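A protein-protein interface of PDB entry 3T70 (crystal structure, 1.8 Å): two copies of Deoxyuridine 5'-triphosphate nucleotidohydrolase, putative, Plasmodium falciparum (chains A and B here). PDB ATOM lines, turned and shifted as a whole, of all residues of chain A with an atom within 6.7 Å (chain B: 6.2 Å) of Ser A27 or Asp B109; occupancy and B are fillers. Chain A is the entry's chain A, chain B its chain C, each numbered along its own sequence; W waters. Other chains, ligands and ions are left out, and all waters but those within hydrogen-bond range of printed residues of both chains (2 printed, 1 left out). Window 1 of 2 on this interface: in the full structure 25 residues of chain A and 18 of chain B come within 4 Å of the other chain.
Of the 11 printed residues of chain B, 4 touch a printed residue of chain A. Hydrophobic or aromatic side chains of chain B that line the printed part of chain A: Leu B107 and Phe B142. Of the 14 printed residues of chain A, 6 touch a printed residue of chain B. Hydrophobic or aromatic side chains of chain A that line the printed part of chain B: Val A140. Among the printed residues, 9 pairs touch across the chains.
Asp B109 touches Asp A26 (OD1 to CA, 3.3 Å). OE1 of Gln A138 touches CD2 of Leu B107, 3.9 Å away. CG2 of Val A140 touches CD2 of Leu B107 (3.9 Å). CG1 of Val A140 touches CE1 of Phe B142, 3.9 Å away. Phe B142 touches Ser A141 (CE1 to O, 3.4 Å). Phe B142 touches Gly A144.
The side-chain hydroxyl (OG) of Ser A27 sits at hydrogen-bond distance from the backbone carbonyl oxygen (O) of Gly A144 (2.6 Å). O of Asp A26 sits at hydrogen-bond distance from N of Leu A147 (3.1 Å). SD of Met A1 lies close to OG of Ser A141.
Of the printed residues of chain B, Ser A27 touches Ser B85 (3.3 Å) and Asp B109 (2.6 Å). Of chain A, only Asp A26 and Ser A27 come within 4 Å of Asp B109. Of the printed residues of chain B, Ser A141 touches Phe B142 (3.4 Å). Of the printed residues of chain A, Leu B107 touches Gln A138 and Val A140. The nearest residue of chain A that does not touch Asp B109 is Gly A25 (4.2 Å).
No position is printed for both chains. Of the 9 pairs that touch across the chains among the printed residues, none has its exchanged pair printed and touching as well.
OG of Ser A27 lies close to OG of Ser B85, 3.4 Å away. The backbone NH (N) of Ser A27 lies within hydrogen-bond range of the side-chain carboxylate (OD1) of Asp B109 (2.6 Å). The side-chain hydroxyl of Ser B85 lies within hydrogen-bond range of the backbone carbonyl oxygen of Gly A144.
Water W1 lies within hydrogen-bond range of the side-chain carboxylate (OD2) of Asp B109 (2.6 Å), the backbone NH (N) of Gly A28 (3.0 Å) and the side-chain amide oxygen (OE1) of Gln A138 (3.5 Å). Water W2 lies within hydrogen-bond range of the side-chain carboxylate of Asp B109 (2.6 Å), the side-chain hydroxyl of Ser A27 (2.7 Å) and the backbone NH of Ala B110 (3.1 Å).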
ATOM      1  N   MET A   1      16.525  11.619  16.984  1.00  0.00           N
ATOM      2  CA  MET A   1      16.724  11.232  18.410  1.00  0.00           C
ATOM      3  C   MET A   1      15.541  11.737  19.221  1.00  0.00           C
ATOM      4  O   MET A   1      15.031  12.828  18.967  1.00  0.00           O
ATOM      5  CB  MET A   1      18.035  11.816  18.955  1.00  0.00           C
ATOM      6  CG  MET A   1      18.425  11.324  20.352  1.00  0.00           C
ATOM      7  SD  MET A   1      19.976  12.020  20.964  1.00  0.00           S
ATOM      8  CE  MET A   1      19.450  13.624  21.566  1.00  0.00           C
ATOM      9  N   GLY A  25      12.210  20.721  12.461  1.00  0.00           N
ATOM     10  CA  GLY A  25      12.990  19.582  12.944  1.00  0.00           C
ATOM     11  C   GLY A  25      14.427  19.977  13.226  1.00  0.00           C
ATOM     12  O   GLY A  25      15.329  19.639  12.462  1.00  0.00           O
ATOM     13  N   ASP A  26      14.639  20.703  14.322  1.00  0.00           N
ATOM     14  CA  ASP A  26      15.962  21.245  14.626  1.00  0.00           C
ATOM     15  C   ASP A  26      16.867  20.182  15.241  1.00  0.00           C
ATOM     16  O   ASP A  26      16.412  19.320  16.001  1.00  0.00           O
ATOM     17  CB  ASP A  26      15.866  22.456  15.562  1.00  0.00           C
ATOM     18  CG  ASP A  26      15.132  23.626  14.939  1.00  0.00           C
ATOM     19  OD1 ASP A  26      15.469  24.013  13.796  1.00  0.00           O
ATOM     20  OD2 ASP A  26      14.223  24.169  15.605  1.00  0.00           O
ATOM     21  N   SER A  27      18.150  20.264  14.901  1.00  0.00           N
ATOM     22  CA  SER A  27      19.169  19.376  15.459  1.00  0.00           C
ATOM     23  C   SER A  27      19.508  19.703  16.913  1.00  0.00           C
ATOM     24  O   SER A  27      20.173  18.923  17.586  1.00  0.00           O
ATOM     25  CB  SER A  27      20.427  19.427  14.596  1.00  0.00           C
ATOM     26  OG  SER A  27      20.151  18.863  13.332  1.00  0.00           O
ATOM     27  N   GLY A  28      19.060  20.861  17.389  1.00  0.00           N
ATOM     28  CA  GLY A  28      19.273  21.244  18.785  1.00  0.00           C
ATOM     29  C   GLY A  28      17.981  21.595  19.486  1.00  0.00           C
ATOM     30  O   GLY A  28      17.147  22.313  18.933  1.00  0.00           O
ATOM     31  N   LEU A  29      17.802  21.070  20.695  1.00  0.00           N
ATOM     32  CA  LEU A  29      16.661  21.433  21.528  1.00  0.00           C
ATOM     33  C   LEU A  29      17.106  22.443  22.568  1.00  0.00           C
ATOM     34  O   LEU A  29      17.887  22.110  23.465  1.00  0.00           O
ATOM     35  CB  LEU A  29      16.085  20.197  22.223  1.00  0.00           C
ATOM     36  CG  LEU A  29      14.870  20.416  23.128  1.00  0.00           C
ATOM     37  CD1 LEU A  29      13.636  20.863  22.319  1.00  0.00           C
ATOM     38  CD2 LEU A  29      14.576  19.137  23.882  1.00  0.00           C
ATOM     39  N   GLN A 138      21.697  24.025  24.537  1.00  0.00           N
ATOM     40  CA  GLN A 138      20.800  23.140  23.791  1.00  0.00           C
ATOM     41  C   GLN A 138      21.326  21.706  23.827  1.00  0.00           C
ATOM     42  O   GLN A 138      22.535  21.477  23.951  1.00  0.00           O
ATOM     43  CB  GLN A 138      20.687  23.616  22.342  1.00  0.00           C
ATOM     44  CG  GLN A 138      22.007  23.610  21.560  1.00  0.00           C
ATOM     45  CD  GLN A 138      21.892  24.247  20.204  1.00  0.00           C
ATOM     46  OE1 GLN A 138      20.865  24.120  19.530  1.00  0.00           O
ATOM     47  NE2 GLN A 138      22.948  24.942  19.783  1.00  0.00           N
ATOM     48  N   LEU A 139      20.413  20.748  23.715  1.00  0.00           N
ATOM     49  CA  LEU A 139      20.797  19.341  23.607  1.00  0.00           C
ATOM     50  C   LEU A 139      20.912  18.952  22.151  1.00  0.00           C
ATOM     51  O   LEU A 139      20.138  19.431  21.313  1.00  0.00           O
ATOM     52  CB  LEU A 139      19.782  18.444  24.323  1.00  0.00           C
ATOM     53  CG  LEU A 139      19.638  18.674  25.829  1.00  0.00           C
ATOM     54  CD1 LEU A 139      18.606  17.708  26.411  1.00  0.00           C
ATOM     55  CD2 LEU A 139      20.994  18.552  26.568  1.00  0.00           C
ATOM     56  N   VAL A 140      21.889  18.098  21.851  1.00  0.00           N
ATOM     57  CA  VAL A 140      22.201  17.716  20.474  1.00  0.00           C
ATOM     58  C   VAL A 140      22.540  16.225  20.421  1.00  0.00           C
ATOM     59  O   VAL A 140      23.182  15.694  21.335  1.00  0.00           O
ATOM     60  CB  VAL A 140      23.395  18.556  19.907  1.00  0.00           C
ATOM     61  CG1 VAL A 140      23.801  18.091  18.504  1.00  0.00           C
ATOM     62  CG2 VAL A 140      23.056  20.059  19.879  1.00  0.00           C
ATOM     63  N   SER A 141      22.094  15.564  19.354  1.00  0.00           N
ATOM     64  CA  SER A 141      22.437  14.165  19.100  1.00  0.00           C
ATOM     65  C   SER A 141      23.805  14.004  18.438  1.00  0.00           C
ATOM     66  O   SER A 141      24.189  14.815  17.597  1.00  0.00           O
ATOM     67  CB  SER A 141      21.369  13.526  18.202  1.00  0.00           C
ATOM     68  OG  SER A 141      21.769  12.222  17.812  1.00  0.00           O
ATOM     69  N   GLY A 144      23.409  14.209  14.826  1.00  0.00           N
ATOM     70  CA  GLY A 144      23.017  15.492  14.257  1.00  0.00           C
ATOM     71  C   GLY A 144      21.609  15.525  13.678  1.00  0.00           C
ATOM     72  O   GLY A 144      21.231  16.505  13.038  1.00  0.00           O
ATOM     73  N   GLU A 145      20.842  14.464  13.919  1.00  0.00           N
ATOM     74  CA  GLU A 145      19.471  14.339  13.409  1.00  0.00           C
ATOM     75  C   GLU A 145      18.499  15.233  14.189  1.00  0.00           C
ATOM     76  O   GLU A 145      18.823  15.674  15.296  1.00  0.00           O
ATOM     77  CB  GLU A 145      19.018  12.868  13.460  1.00  0.00           C
ATOM     78  CG  GLU A 145      18.727  12.331  14.868  1.00  0.00           C
ATOM     79  CD  GLU A 145      18.970  10.829  15.016  1.00  0.00           C
ATOM     80  OE1 GLU A 145      18.640  10.279  16.078  1.00  0.00           O
ATOM     81  OE2 GLU A 145      19.509  10.197  14.082  1.00  0.00           O
ATOM     82  N   PRO A 146      17.309  15.514  13.610  1.00  0.00           N
ATOM     83  CA  PRO A 146      16.242  16.227  14.328  1.00  0.00           C
ATOM     84  C   PRO A 146      15.890  15.605  15.684  1.00  0.00           C
ATOM     85  O   PRO A 146      15.965  14.379  15.862  1.00  0.00           O
ATOM     86  CB  PRO A 146      15.044  16.114  13.377  1.00  0.00           C
ATOM     87  CG  PRO A 146      15.652  16.015  12.037  1.00  0.00           C
ATOM     88  CD  PRO A 146      16.902  15.216  12.218  1.00  0.00           C
ATOM     89  N   LEU A 147      15.524  16.459  16.631  1.00  0.00           N
ATOM     90  CA  LEU A 147      15.198  16.011  17.976  1.00  0.00           C
ATOM     91  C   LEU A 147      13.730  16.221  18.270  1.00  0.00           C
ATOM     92  O   LEU A 147      13.176  17.289  17.988  1.00  0.00           O
ATOM     93  CB  LEU A 147      16.015  16.776  19.021  1.00  0.00           C
ATOM     94  CG  LEU A 147      17.539  16.788  18.977  1.00  0.00           C
ATOM     95  CD1 LEU A 147      18.014  17.154  20.361  1.00  0.00           C
ATOM     96  CD2 LEU A 147      18.149  15.462  18.538  1.00  0.00           C
ATOM     97  N   THR B  84      21.666  17.904   5.422  1.00  0.00           N
ATOM     98  CA  THR B  84      21.986  17.506   6.784  1.00  0.00           C
ATOM     99  C   THR B  84      22.603  18.658   7.568  1.00  0.00           C
ATOM    100  O   THR B  84      23.132  19.603   6.985  1.00  0.00           O
ATOM    101  CB  THR B  84      22.898  16.248   6.824  1.00  0.00           C
ATOM    102  OG1 THR B  84      23.158  15.870   8.183  1.00  0.00           O
ATOM    103  CG2 THR B  84      24.217  16.496   6.107  1.00  0.00           C
ATOM    104  N   SER B  85      22.493  18.561   8.889  1.00  0.00           N
ATOM    105  CA  SER B  85      23.176  19.457   9.806  1.00  0.00           C
ATOM    106  C   SER B  85      24.674  19.181   9.769  1.00  0.00           C
ATOM    107  O   SER B  85      25.102  18.083   9.393  1.00  0.00           O
ATOM    108  CB  SER B  85      22.663  19.220  11.224  1.00  0.00           C
ATOM    109  OG  SER B  85      22.906  17.880  11.617  1.00  0.00           O
ATOM    110  N   PHE B  86      25.469  20.168  10.168  1.00  0.00           N
ATOM    111  CA  PHE B  86      26.908  19.971  10.256  1.00  0.00           C
ATOM    112  C   PHE B  86      27.496  20.928  11.276  1.00  0.00           C
ATOM    113  O   PHE B  86      26.760  21.702  11.914  1.00  0.00           O
ATOM    114  CB  PHE B  86      27.595  20.084   8.883  1.00  0.00           C
ATOM    115  CG  PHE B  86      27.346  21.385   8.171  1.00  0.00           C
ATOM    116  CD1 PHE B  86      26.153  21.603   7.480  1.00  0.00           C
ATOM    117  CD2 PHE B  86      28.314  22.395   8.179  1.00  0.00           C
ATOM    118  CE1 PHE B  86      25.916  22.802   6.815  1.00  0.00           C
ATOM    119  CE2 PHE B  86      28.085  23.609   7.516  1.00  0.00           C
ATOM    120  CZ  PHE B  86      26.893  23.808   6.825  1.00  0.00           C
ATOM    121  N   LEU B 107      26.814  24.907  15.432  1.00  0.00           N
ATOM    122  CA  LEU B 107      25.854  23.946  14.905  1.00  0.00           C
ATOM    123  C   LEU B 107      25.105  24.592  13.756  1.00  0.00           C
ATOM    124  O   LEU B 107      24.450  25.615  13.935  1.00  0.00           O
ATOM    125  CB  LEU B 107      24.855  23.520  15.982  1.00  0.00           C
ATOM    126  CG  LEU B 107      23.725  22.589  15.521  1.00  0.00           C
ATOM    127  CD1 LEU B 107      24.280  21.296  14.913  1.00  0.00           C
ATOM    128  CD2 LEU B 107      22.757  22.296  16.665  1.00  0.00           C
ATOM    129  N   ILE B 108      25.209  23.999  12.577  1.00  0.00           N
ATOM    130  CA  ILE B 108      24.489  24.537  11.432  1.00  0.00           C
ATOM    131  C   ILE B 108      23.424  23.524  11.068  1.00  0.00           C
ATOM    132  O   ILE B 108      23.740  22.399  10.695  1.00  0.00           O
ATOM    133  CB  ILE B 108      25.431  24.863  10.256  1.00  0.00           C
ATOM    134  CG1 ILE B 108      26.356  26.013  10.659  1.00  0.00           C
ATOM    135  CG2 ILE B 108      24.624  25.309   9.034  1.00  0.00           C
ATOM    136  CD1 ILE B 108      27.751  25.827  10.222  1.00  0.00           C
ATOM    137  N   ASP B 109      22.167  23.921  11.227  1.00  0.00           N
ATOM    138  CA  ASP B 109      21.054  23.017  10.980  1.00  0.00           C
ATOM    139  C   ASP B 109      20.859  22.726   9.493  1.00  0.00           C
ATOM    140  O   ASP B 109      21.207  23.546   8.642  1.00  0.00           O
ATOM    141  CB  ASP B 109      19.771  23.550  11.608  1.00  0.00           C
ATOM    142  CG  ASP B 109      19.512  22.958  12.972  1.00  0.00           C
ATOM    143  OD1 ASP B 109      18.801  21.934  13.023  1.00  0.00           O
ATOM    144  OD2 ASP B 109      20.037  23.482  13.983  1.00  0.00           O
ATOM    145  N   ALA B 110      20.324  21.540   9.212  1.00  0.00           N
ATOM    146  CA  ALA B 110      20.031  21.089   7.862  1.00  0.00           C
ATOM    147  C   ALA B 110      19.304  22.188   7.113  1.00  0.00           C
ATOM    148  O   ALA B 110      18.320  22.747   7.604  1.00  0.00           O
ATOM    149  CB  ALA B 110      19.190  19.811   7.889  1.00  0.00           C
ATOM    150  N   GLY B 111      19.832  22.524   5.943  1.00  0.00           N
ATOM    151  CA  GLY B 111      19.207  23.502   5.066  1.00  0.00           C
ATOM    152  C   GLY B 111      19.362  24.974   5.421  1.00  0.00           C
ATOM    153  O   GLY B 111      18.804  25.813   4.720  1.00  0.00           O
ATOM    154  N   TYR B 112      20.103  25.298   6.495  1.00  0.00           N
ATOM    155  CA  TYR B 112      20.372  26.695   6.861  1.00  0.00           C
ATOM    156  C   TYR B 112      20.951  27.443   5.657  1.00  0.00           C
ATOM    157  O   TYR B 112      21.844  26.928   4.989  1.00  0.00           O
ATOM    158  CB  TYR B 112      21.344  26.785   8.051  1.00  0.00           C
ATOM    159  CG  TYR B 112      21.696  28.198   8.452  1.00  0.00           C
ATOM    160  CD1 TYR B 112      20.747  29.025   9.051  1.00  0.00           C
ATOM    161  CD2 TYR B 112      22.983  28.708   8.243  1.00  0.00           C
ATOM    162  CE1 TYR B 112      21.057  30.319   9.420  1.00  0.00           C
ATOM    163  CE2 TYR B 112      23.305  30.011   8.614  1.00  0.00           C
ATOM    164  CZ  TYR B 112      22.332  30.806   9.201  1.00  0.00           C
ATOM    165  OH  TYR B 112      22.618  32.087   9.581  1.00  0.00           O
ATOM    166  N   ARG B 113      20.428  28.637   5.382  1.00  0.00           N
ATOM    167  CA  ARG B 113      20.781  29.390   4.169  1.00  0.00           C
ATOM    168  C   ARG B 113      21.520  30.710   4.420  1.00  0.00           C
ATOM    169  O   ARG B 113      21.819  31.444   3.477  1.00  0.00           O
ATOM    170  CB  ARG B 113      19.523  29.655   3.322  1.00  0.00           C
ATOM    171  CG  ARG B 113      18.920  28.408   2.688  1.00  0.00           C
ATOM    172  CD  ARG B 113      17.424  28.313   2.968  1.00  0.00           C
ATOM    173  NE  ARG B 113      16.657  29.410   2.383  1.00  0.00           N
ATOM    174  CZ  ARG B 113      15.480  29.839   2.838  1.00  0.00           C
ATOM    175  NH1 ARG B 113      14.920  29.273   3.904  1.00  0.00           N
ATOM    176  NH2 ARG B 113      14.861  30.847   2.229  1.00  0.00           N
ATOM    177  N   PHE B 142      28.898  15.303  11.297  1.00  0.00           N
ATOM    178  CA  PHE B 142      28.530  14.547  12.501  1.00  0.00           C
ATOM    179  C   PHE B 142      29.046  13.095  12.496  1.00  0.00           C
ATOM    180  O   PHE B 142      29.202  12.483  13.550  1.00  0.00           O
ATOM    181  CB  PHE B 142      27.011  14.555  12.696  1.00  0.00           C
ATOM    182  CG  PHE B 142      26.499  15.763  13.431  1.00  0.00           C
ATOM    183  CD1 PHE B 142      26.457  15.774  14.827  1.00  0.00           C
ATOM    184  CD2 PHE B 142      26.055  16.889  12.731  1.00  0.00           C
ATOM    185  CE1 PHE B 142      25.980  16.885  15.521  1.00  0.00           C
ATOM    186  CE2 PHE B 142      25.570  18.001  13.410  1.00  0.00           C
ATOM    187  CZ  PHE B 142      25.538  17.998  14.814  1.00  0.00           C
HETATM  188  O   HOH W   1      19.315  23.669  16.430  1.00  0.00           O
HETATM  189  O   HOH W   2      18.744  19.977  11.360  1.00  0.00           O
